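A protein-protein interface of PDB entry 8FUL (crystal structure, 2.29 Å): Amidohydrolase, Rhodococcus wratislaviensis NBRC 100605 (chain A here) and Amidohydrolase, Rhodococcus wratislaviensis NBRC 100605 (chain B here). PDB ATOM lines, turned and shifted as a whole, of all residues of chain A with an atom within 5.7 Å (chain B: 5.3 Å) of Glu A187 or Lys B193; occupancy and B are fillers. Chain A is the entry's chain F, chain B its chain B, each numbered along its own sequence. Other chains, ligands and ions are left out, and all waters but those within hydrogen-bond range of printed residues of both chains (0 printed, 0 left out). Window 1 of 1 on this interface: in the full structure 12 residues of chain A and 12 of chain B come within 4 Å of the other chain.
Printed residues of chain A that touch a printed residue of chain B: Leu A186, Glu A187 and Lys A193.
Hydrophobic or aromatic side chains of chain B within 4 Å of the printed part of chain A: Leu B186.
Among the printed residues, Asp or Glu carboxylates within 4 Å of a Lys or Arg side-chain nitrogen of the other chain: Glu A187 with Lys B193 (2.9 Å) and Lys A193 with Glu B187 (2.9 Å).
Among the printed residues, pairs that only touch across the chains: Glu A187 with Leu B186 (3.2 Å), Leu A186 with Glu B187 (3.5 Å) and Leu A186 with Leu B186 (3.9 Å).
Of chain B, only Leu B186 (3.2 Å) and Lys B193 (2.9 Å) come within 4 Å of Glu A187.
Lys B193 touches just one residue of chain A: Glu A187 (2.9 Å).
Printed residues of chain A within 4 Å of Glu B187: Leu A186 (3.5 Å) and Lys A193 (2.9 Å).
Of the printed residues of chain B, Lys A193 touches Glu B187 (2.9 Å).
Of the printed residues of chain A, Leu B186 touches Leu A186 and Glu A187.
The nearest residue of chain B that does not touch Glu A187 is Glu B187 (4.9 Å).
The backbone NH (N) of Lys A193 sits close to the side-chain hydroxyl (OG) of Ser A191 (3.1 Å).
The backbone carbonyl oxygen of Leu A186 sits at hydrogen-bond distance from a ring nitrogen (NE2) of His A218, 2.4 Å away.
The backbone carbonyl oxygen (O) of Glu B187 is in hydrogen-bond range of the side-chain hydroxyl (OH) of Tyr B194 (3.1 Å).
The backbone carbonyl oxygen (O) of Gly A216 sits at hydrogen-bond distance from the backbone NH (N) of Leu A186, at 3.3 Å.
OE2 of Glu A158 is in hydrogen-bond range of N of Leu A186, at 2.9 Å.
The side-chain carboxylate (OE1) of Glu A187 is in hydrogen-bond range of the side-chain hydroxyl (OG) of Ser A191 (3.1 Å).
NZ of Lys A193 lies within salt-bridge range of OE2 of Glu B187 (2.9 Å).
The side-chain carboxylate (OE2) of Glu A187 is in salt-bridge range of the side-chain amino group (NZ) of Lys B193.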
ATOM      1  N   GLU A 158       8.342  26.554  -4.097  1.00  0.00           N
ATOM      2  CA  GLU A 158       9.380  25.661  -4.606  1.00  0.00           C
ATOM      3  C   GLU A 158      10.399  26.350  -5.500  1.00  0.00           C
ATOM      4  O   GLU A 158      11.383  25.714  -5.870  1.00  0.00           O
ATOM      5  CB  GLU A 158       8.786  24.475  -5.381  1.00  0.00           C
ATOM      6  CG  GLU A 158       7.904  23.525  -4.558  1.00  0.00           C
ATOM      7  CD  GLU A 158       8.587  22.948  -3.313  1.00  0.00           C
ATOM      8  OE1 GLU A 158       9.835  22.987  -3.188  1.00  0.00           O
ATOM      9  OE2 GLU A 158       7.854  22.440  -2.444  1.00  0.00           O
ATOM     10  N   THR A 185       4.877  20.151   0.592  1.00  0.00           N
ATOM     11  CA  THR A 185       6.026  20.761  -0.034  1.00  0.00           C
ATOM     12  C   THR A 185       7.047  19.656  -0.231  1.00  0.00           C
ATOM     13  O   THR A 185       6.959  18.596   0.409  1.00  0.00           O
ATOM     14  CB  THR A 185       6.595  21.875   0.856  1.00  0.00           C
ATOM     15  OG1 THR A 185       6.604  21.398   2.205  1.00  0.00           O
ATOM     16  CG2 THR A 185       5.760  23.187   0.772  1.00  0.00           C
ATOM     17  N   LEU A 186       8.040  19.933  -1.095  1.00  0.00           N
ATOM     18  CA  LEU A 186       9.075  18.947  -1.387  1.00  0.00           C
ATOM     19  C   LEU A 186       9.934  18.678  -0.165  1.00  0.00           C
ATOM     20  O   LEU A 186      10.347  17.536   0.074  1.00  0.00           O
ATOM     21  CB  LEU A 186       9.936  19.423  -2.555  1.00  0.00           C
ATOM     22  CG  LEU A 186      10.823  18.349  -3.192  1.00  0.00           C
ATOM     23  CD1 LEU A 186       9.974  17.178  -3.760  1.00  0.00           C
ATOM     24  CD2 LEU A 186      11.716  18.948  -4.260  1.00  0.00           C
ATOM     25  N   GLU A 187      10.223  19.713   0.613  1.00  0.00           N
ATOM     26  CA  GLU A 187      10.912  19.532   1.878  1.00  0.00           C
ATOM     27  C   GLU A 187      10.149  20.270   2.965  1.00  0.00           C
ATOM     28  O   GLU A 187       9.404  21.215   2.675  1.00  0.00           O
ATOM     29  CB  GLU A 187      12.365  20.040   1.835  1.00  0.00           C
ATOM     30  CG  GLU A 187      13.012  20.076   0.470  1.00  0.00           C
ATOM     31  CD  GLU A 187      14.381  20.747   0.499  1.00  0.00           C
ATOM     32  OE1 GLU A 187      14.988  20.847   1.590  1.00  0.00           O
ATOM     33  OE2 GLU A 187      14.845  21.175  -0.573  1.00  0.00           O
ATOM     34  N   PRO A 188      10.307  19.860   4.224  1.00  0.00           N
ATOM     35  CA  PRO A 188       9.530  20.487   5.293  1.00  0.00           C
ATOM     36  C   PRO A 188       9.829  21.976   5.416  1.00  0.00           C
ATOM     37  O   PRO A 188      10.928  22.441   5.104  1.00  0.00           O
ATOM     38  CB  PRO A 188       9.965  19.704   6.532  1.00  0.00           C
ATOM     39  CG  PRO A 188      10.281  18.361   5.999  1.00  0.00           C
ATOM     40  CD  PRO A 188      11.038  18.686   4.725  1.00  0.00           C
ATOM     41  N   LEU A 189       8.817  22.725   5.863  1.00  0.00           N
ATOM     42  CA  LEU A 189       8.805  24.183   5.701  1.00  0.00           C
ATOM     43  C   LEU A 189       9.859  24.900   6.541  1.00  0.00           C
ATOM     44  O   LEU A 189      10.151  26.072   6.273  1.00  0.00           O
ATOM     45  CB  LEU A 189       7.428  24.734   6.050  1.00  0.00           C
ATOM     46  CG  LEU A 189       6.322  24.579   5.023  1.00  0.00           C
ATOM     47  CD1 LEU A 189       4.960  24.912   5.662  1.00  0.00           C
ATOM     48  CD2 LEU A 189       6.631  25.459   3.834  1.00  0.00           C
ATOM     49  N   SER A 191      12.896  24.113   6.389  1.00  0.00           N
ATOM     50  CA  SER A 191      14.160  23.932   5.688  1.00  0.00           C
ATOM     51  C   SER A 191      14.687  25.268   5.178  1.00  0.00           C
ATOM     52  O   SER A 191      13.921  26.186   4.867  1.00  0.00           O
ATOM     53  CB  SER A 191      13.993  22.956   4.528  1.00  0.00           C
ATOM     54  OG  SER A 191      14.861  23.279   3.454  1.00  0.00           O
ATOM     55  N   LYS A 193      15.720  26.037   2.403  1.00  0.00           N
ATOM     56  CA  LYS A 193      15.255  26.374   1.059  1.00  0.00           C
ATOM     57  C   LYS A 193      14.292  27.556   1.070  1.00  0.00           C
ATOM     58  O   LYS A 193      14.377  28.449   0.217  1.00  0.00           O
ATOM     59  CB  LYS A 193      14.595  25.150   0.416  1.00  0.00           C
ATOM     60  CG  LYS A 193      13.981  25.432  -0.985  1.00  0.00           C
ATOM     61  CD  LYS A 193      13.412  24.190  -1.659  1.00  0.00           C
ATOM     62  CE  LYS A 193      12.770  24.565  -2.975  1.00  0.00           C
ATOM     63  NZ  LYS A 193      12.361  23.416  -3.831  1.00  0.00           N
ATOM     64  N   TYR A 194      13.393  27.597   2.056  1.00  0.00           N
ATOM     65  CA  TYR A 194      12.280  28.534   2.113  1.00  0.00           C
ATOM     66  C   TYR A 194      12.603  29.826   2.860  1.00  0.00           C
ATOM     67  O   TYR A 194      11.781  30.754   2.865  1.00  0.00           O
ATOM     68  CB  TYR A 194      11.087  27.832   2.765  1.00  0.00           C
ATOM     69  CG  TYR A 194      10.755  26.540   2.067  1.00  0.00           C
ATOM     70  CD1 TYR A 194      10.258  26.548   0.767  1.00  0.00           C
ATOM     71  CD2 TYR A 194      10.977  25.311   2.686  1.00  0.00           C
ATOM     72  CE1 TYR A 194       9.959  25.372   0.110  1.00  0.00           C
ATOM     73  CE2 TYR A 194      10.685  24.119   2.034  1.00  0.00           C
ATOM     74  CZ  TYR A 194      10.180  24.156   0.747  1.00  0.00           C
ATOM     75  OH  TYR A 194       9.894  22.990   0.077  1.00  0.00           O
ATOM     76  N   GLY A 216       2.895  18.275  -3.695  1.00  0.00           N
ATOM     77  CA  GLY A 216       4.103  18.439  -2.927  1.00  0.00           C
ATOM     78  C   GLY A 216       5.288  17.644  -3.449  1.00  0.00           C
ATOM     79  O   GLY A 216       6.437  18.068  -3.270  1.00  0.00           O
ATOM     80  N   HIS A 218       5.648  14.185  -2.652  1.00  0.00           N
ATOM     81  CA  HIS A 218       5.619  12.965  -1.870  1.00  0.00           C
ATOM     82  C   HIS A 218       4.167  12.519  -1.694  1.00  0.00           C
ATOM     83  O   HIS A 218       3.225  13.280  -1.935  1.00  0.00           O
ATOM     84  CB  HIS A 218       6.267  13.179  -0.493  1.00  0.00           C
ATOM     85  CG  HIS A 218       7.528  13.996  -0.522  1.00  0.00           C
ATOM     86  ND1 HIS A 218       8.784  13.429  -0.615  1.00  0.00           N
ATOM     87  CD2 HIS A 218       7.724  15.334  -0.438  1.00  0.00           C
ATOM     88  CE1 HIS A 218       9.698  14.382  -0.584  1.00  0.00           C
ATOM     89  NE2 HIS A 218       9.082  15.547  -0.486  1.00  0.00           N
ATOM     90  N   GLN A 243       4.670  19.968   9.215  1.00  0.00           N
ATOM     91  CA  GLN A 243       5.174  21.313   8.973  1.00  0.00           C
ATOM     92  C   GLN A 243       5.354  22.086  10.276  1.00  0.00           C
ATOM     93  O   GLN A 243       6.337  22.814  10.428  1.00  0.00           O
ATOM     94  CB  GLN A 243       4.256  22.061   8.018  1.00  0.00           C
ATOM     95  CG  GLN A 243       4.025  21.422   6.643  1.00  0.00           C
ATOM     96  CD  GLN A 243       5.220  21.453   5.700  1.00  0.00           C
ATOM     97  OE1 GLN A 243       6.363  21.291   6.121  1.00  0.00           O
ATOM     98  NE2 GLN A 243       4.949  21.642   4.397  1.00  0.00           N
ATOM     99  N   PHE B 157      25.067  19.782  -2.143  1.00  0.00           N
ATOM    100  CA  PHE B 157      24.279  20.275  -3.272  1.00  0.00           C
ATOM    101  C   PHE B 157      22.867  20.640  -2.863  1.00  0.00           C
ATOM    102  O   PHE B 157      22.244  21.514  -3.487  1.00  0.00           O
ATOM    103  CB  PHE B 157      24.264  19.258  -4.416  1.00  0.00           C
ATOM    104  CG  PHE B 157      25.316  19.522  -5.430  1.00  0.00           C
ATOM    105  CD1 PHE B 157      26.647  19.289  -5.131  1.00  0.00           C
ATOM    106  CD2 PHE B 157      24.988  20.059  -6.662  1.00  0.00           C
ATOM    107  CE1 PHE B 157      27.631  19.565  -6.050  1.00  0.00           C
ATOM    108  CE2 PHE B 157      25.973  20.336  -7.584  1.00  0.00           C
ATOM    109  CZ  PHE B 157      27.296  20.089  -7.274  1.00  0.00           C
ATOM    110  N   GLU B 158      22.366  20.015  -1.803  1.00  0.00           N
ATOM    111  CA  GLU B 158      21.020  20.285  -1.327  1.00  0.00           C
ATOM    112  C   GLU B 158      20.931  21.501  -0.415  1.00  0.00           C
ATOM    113  O   GLU B 158      19.819  21.881  -0.052  1.00  0.00           O
ATOM    114  CB  GLU B 158      20.470  19.044  -0.614  1.00  0.00           C
ATOM    115  CG  GLU B 158      20.608  17.755  -1.404  1.00  0.00           C
ATOM    116  CD  GLU B 158      19.708  17.663  -2.644  1.00  0.00           C
ATOM    117  OE1 GLU B 158      19.071  18.660  -3.037  1.00  0.00           O
ATOM    118  OE2 GLU B 158      19.616  16.555  -3.218  1.00  0.00           O
ATOM    119  N   THR B 159      22.054  22.117  -0.035  1.00  0.00           N
ATOM    120  CA  THR B 159      22.046  23.429   0.617  1.00  0.00           C
ATOM    121  C   THR B 159      22.941  24.364  -0.169  1.00  0.00           C
ATOM    122  O   THR B 159      24.134  24.466   0.126  1.00  0.00           O
ATOM    123  CB  THR B 159      22.540  23.361   2.056  1.00  0.00           C
ATOM    124  OG1 THR B 159      21.800  22.370   2.759  1.00  0.00           O
ATOM    125  CG2 THR B 159      22.356  24.730   2.737  1.00  0.00           C
ATOM    126  N   PRO B 160      22.416  25.024  -1.198  1.00  0.00           N
ATOM    127  CA  PRO B 160      23.286  25.849  -2.067  1.00  0.00           C
ATOM    128  C   PRO B 160      24.152  26.864  -1.330  1.00  0.00           C
ATOM    129  O   PRO B 160      25.332  27.009  -1.675  1.00  0.00           O
ATOM    130  CB  PRO B 160      22.276  26.525  -2.995  1.00  0.00           C
ATOM    131  CG  PRO B 160      21.196  25.480  -3.144  1.00  0.00           C
ATOM    132  CD  PRO B 160      21.095  24.778  -1.808  1.00  0.00           C
ATOM    133  N   LEU B 186      17.422  15.558  -4.599  1.00  0.00           N
ATOM    134  CA  LEU B 186      15.990  15.732  -4.310  1.00  0.00           C
ATOM    135  C   LEU B 186      15.236  16.313  -5.502  1.00  0.00           C
ATOM    136  O   LEU B 186      14.065  15.985  -5.702  1.00  0.00           O
ATOM    137  CB  LEU B 186      15.786  16.624  -3.082  1.00  0.00           C
ATOM    138  CG  LEU B 186      14.371  16.742  -2.455  1.00  0.00           C
ATOM    139  CD1 LEU B 186      13.729  15.425  -1.940  1.00  0.00           C
ATOM    140  CD2 LEU B 186      14.383  17.760  -1.315  1.00  0.00           C
ATOM    141  N   GLU B 187      15.870  17.179  -6.296  1.00  0.00           N
ATOM    142  CA  GLU B 187      15.273  17.581  -7.555  1.00  0.00           C
ATOM    143  C   GLU B 187      16.278  17.401  -8.683  1.00  0.00           C
ATOM    144  O   GLU B 187      17.491  17.444  -8.463  1.00  0.00           O
ATOM    145  CB  GLU B 187      14.798  19.036  -7.545  1.00  0.00           C
ATOM    146  CG  GLU B 187      14.507  19.659  -6.217  1.00  0.00           C
ATOM    147  CD  GLU B 187      14.096  21.129  -6.381  1.00  0.00           C
ATOM    148  OE1 GLU B 187      13.641  21.506  -7.482  1.00  0.00           O
ATOM    149  OE2 GLU B 187      14.241  21.899  -5.418  1.00  0.00           O
ATOM    150  N   SER B 191      17.327  21.871 -12.162  1.00  0.00           N
ATOM    151  CA  SER B 191      16.450  22.765 -11.421  1.00  0.00           C
ATOM    152  C   SER B 191      17.225  23.989 -10.960  1.00  0.00           C
ATOM    153  O   SER B 191      18.449  23.954 -10.818  1.00  0.00           O
ATOM    154  CB  SER B 191      15.835  22.062 -10.209  1.00  0.00           C
ATOM    155  OG  SER B 191      15.053  22.969  -9.440  1.00  0.00           O
ATOM    156  N   ARG B 192      16.483  25.078 -10.715  1.00  0.00           N
ATOM    157  CA  ARG B 192      17.087  26.349 -10.314  1.00  0.00           C
ATOM    158  C   ARG B 192      17.686  26.280  -8.921  1.00  0.00           C
ATOM    159  O   ARG B 192      18.543  27.105  -8.577  1.00  0.00           O
ATOM    160  CB  ARG B 192      16.043  27.474 -10.380  1.00  0.00           C
ATOM    161  CG  ARG B 192      16.598  28.865 -10.071  1.00  0.00           C
ATOM    162  CD  ARG B 192      15.561  30.000 -10.108  1.00  0.00           C
ATOM    163  NE  ARG B 192      16.139  31.184 -10.745  1.00  0.00           N
ATOM    164  CZ  ARG B 192      16.240  31.347 -12.066  1.00  0.00           C
ATOM    165  NH1 ARG B 192      16.792  32.447 -12.552  1.00  0.00           N
ATOM    166  NH2 ARG B 192      15.785  30.425 -12.907  1.00  0.00           N
ATOM    167  N   LYS B 193      17.285  25.296  -8.119  1.00  0.00           N
ATOM    168  CA  LYS B 193      17.858  25.152  -6.794  1.00  0.00           C
ATOM    169  C   LYS B 193      19.378  25.103  -6.859  1.00  0.00           C
ATOM    170  O   LYS B 193      20.057  25.665  -5.998  1.00  0.00           O
ATOM    171  CB  LYS B 193      17.309  23.900  -6.126  1.00  0.00           C
ATOM    172  CG  LYS B 193      17.917  23.617  -4.782  1.00  0.00           C
ATOM    173  CD  LYS B 193      17.421  22.308  -4.226  1.00  0.00           C
ATOM    174  CE  LYS B 193      18.240  21.914  -3.017  1.00  0.00           C
ATOM    175  NZ  LYS B 193      17.386  21.192  -2.033  1.00  0.00           N
ATOM    176  N   TYR B 194      19.929  24.469  -7.891  1.00  0.00           N
ATOM    177  CA  TYR B 194      21.361  24.179  -7.951  1.00  0.00           C
ATOM    178  C   TYR B 194      22.147  25.253  -8.669  1.00  0.00           C
ATOM    179  O   TYR B 194      23.381  25.268  -8.577  1.00  0.00           O
ATOM    180  CB  TYR B 194      21.601  22.814  -8.633  1.00  0.00           C
ATOM    181  CG  TYR B 194      20.833  21.714  -7.940  1.00  0.00           C
ATOM    182  CD1 TYR B 194      21.173  21.319  -6.642  1.00  0.00           C
ATOM    183  CD2 TYR B 194      19.741  21.117  -8.549  1.00  0.00           C
ATOM    184  CE1 TYR B 194      20.473  20.339  -5.986  1.00  0.00           C
ATOM    185  CE2 TYR B 194      19.010  20.124  -7.890  1.00  0.00           C
ATOM    186  CZ  TYR B 194      19.386  19.741  -6.615  1.00  0.00           C
ATOM    187  OH  TYR B 194      18.670  18.776  -5.951  1.00  0.00           O
ATOM    188  N   TRP B 195      21.456  26.133  -9.373  1.00  0.00           N
ATOM    189  CA  TRP B 195      22.106  27.168 -10.164  1.00  0.00           C
ATOM    190  C   TRP B 195      23.092  28.020  -9.366  1.00  0.00           C
ATOM    191  O   TRP B 195      24.162  28.336  -9.906  1.00  0.00           O
ATOM    192  CB  TRP B 195      21.000  28.010 -10.825  1.00  0.00           C
ATOM    193  CG  TRP B 195      20.386  27.326 -11.999  1.00  0.00           C
ATOM    194  CD1 TRP B 195      20.374  25.984 -12.247  1.00  0.00           C
ATOM    195  CD2 TRP B 195      19.744  27.945 -13.121  1.00  0.00           C
ATOM    196  NE1 TRP B 195      19.741  25.725 -13.440  1.00  0.00           N
ATOM    197  CE2 TRP B 195      19.353  26.906 -14.004  1.00  0.00           C
ATOM    198  CE3 TRP B 195      19.447  29.277 -13.464  1.00  0.00           C
ATOM    199  CZ2 TRP B 195      18.685  27.150 -15.200  1.00  0.00           C
ATOM    200  CZ3 TRP B 195      18.789  29.519 -14.676  1.00  0.00           C
ATOM    201  CH2 TRP B 195      18.426  28.463 -15.522  1.00  0.00           C
ATOM    202  N   PRO B 196      22.814  28.425  -8.123  1.00  0.00           N
ATOM    203  CA  PRO B 196      23.843  29.143  -7.355  1.00  0.00           C
ATOM    204  C   PRO B 196      25.146  28.391  -7.223  1.00  0.00           C
ATOM    205  O   PRO B 196      26.191  29.030  -7.054  1.00  0.00           O
ATOM    206  CB  PRO B 196      23.170  29.358  -5.986  1.00  0.00           C
ATOM    207  CG  PRO B 196      21.735  29.500  -6.316  1.00  0.00           C
ATOM    208  CD  PRO B 196      21.481  28.571  -7.499  1.00  0.00           C
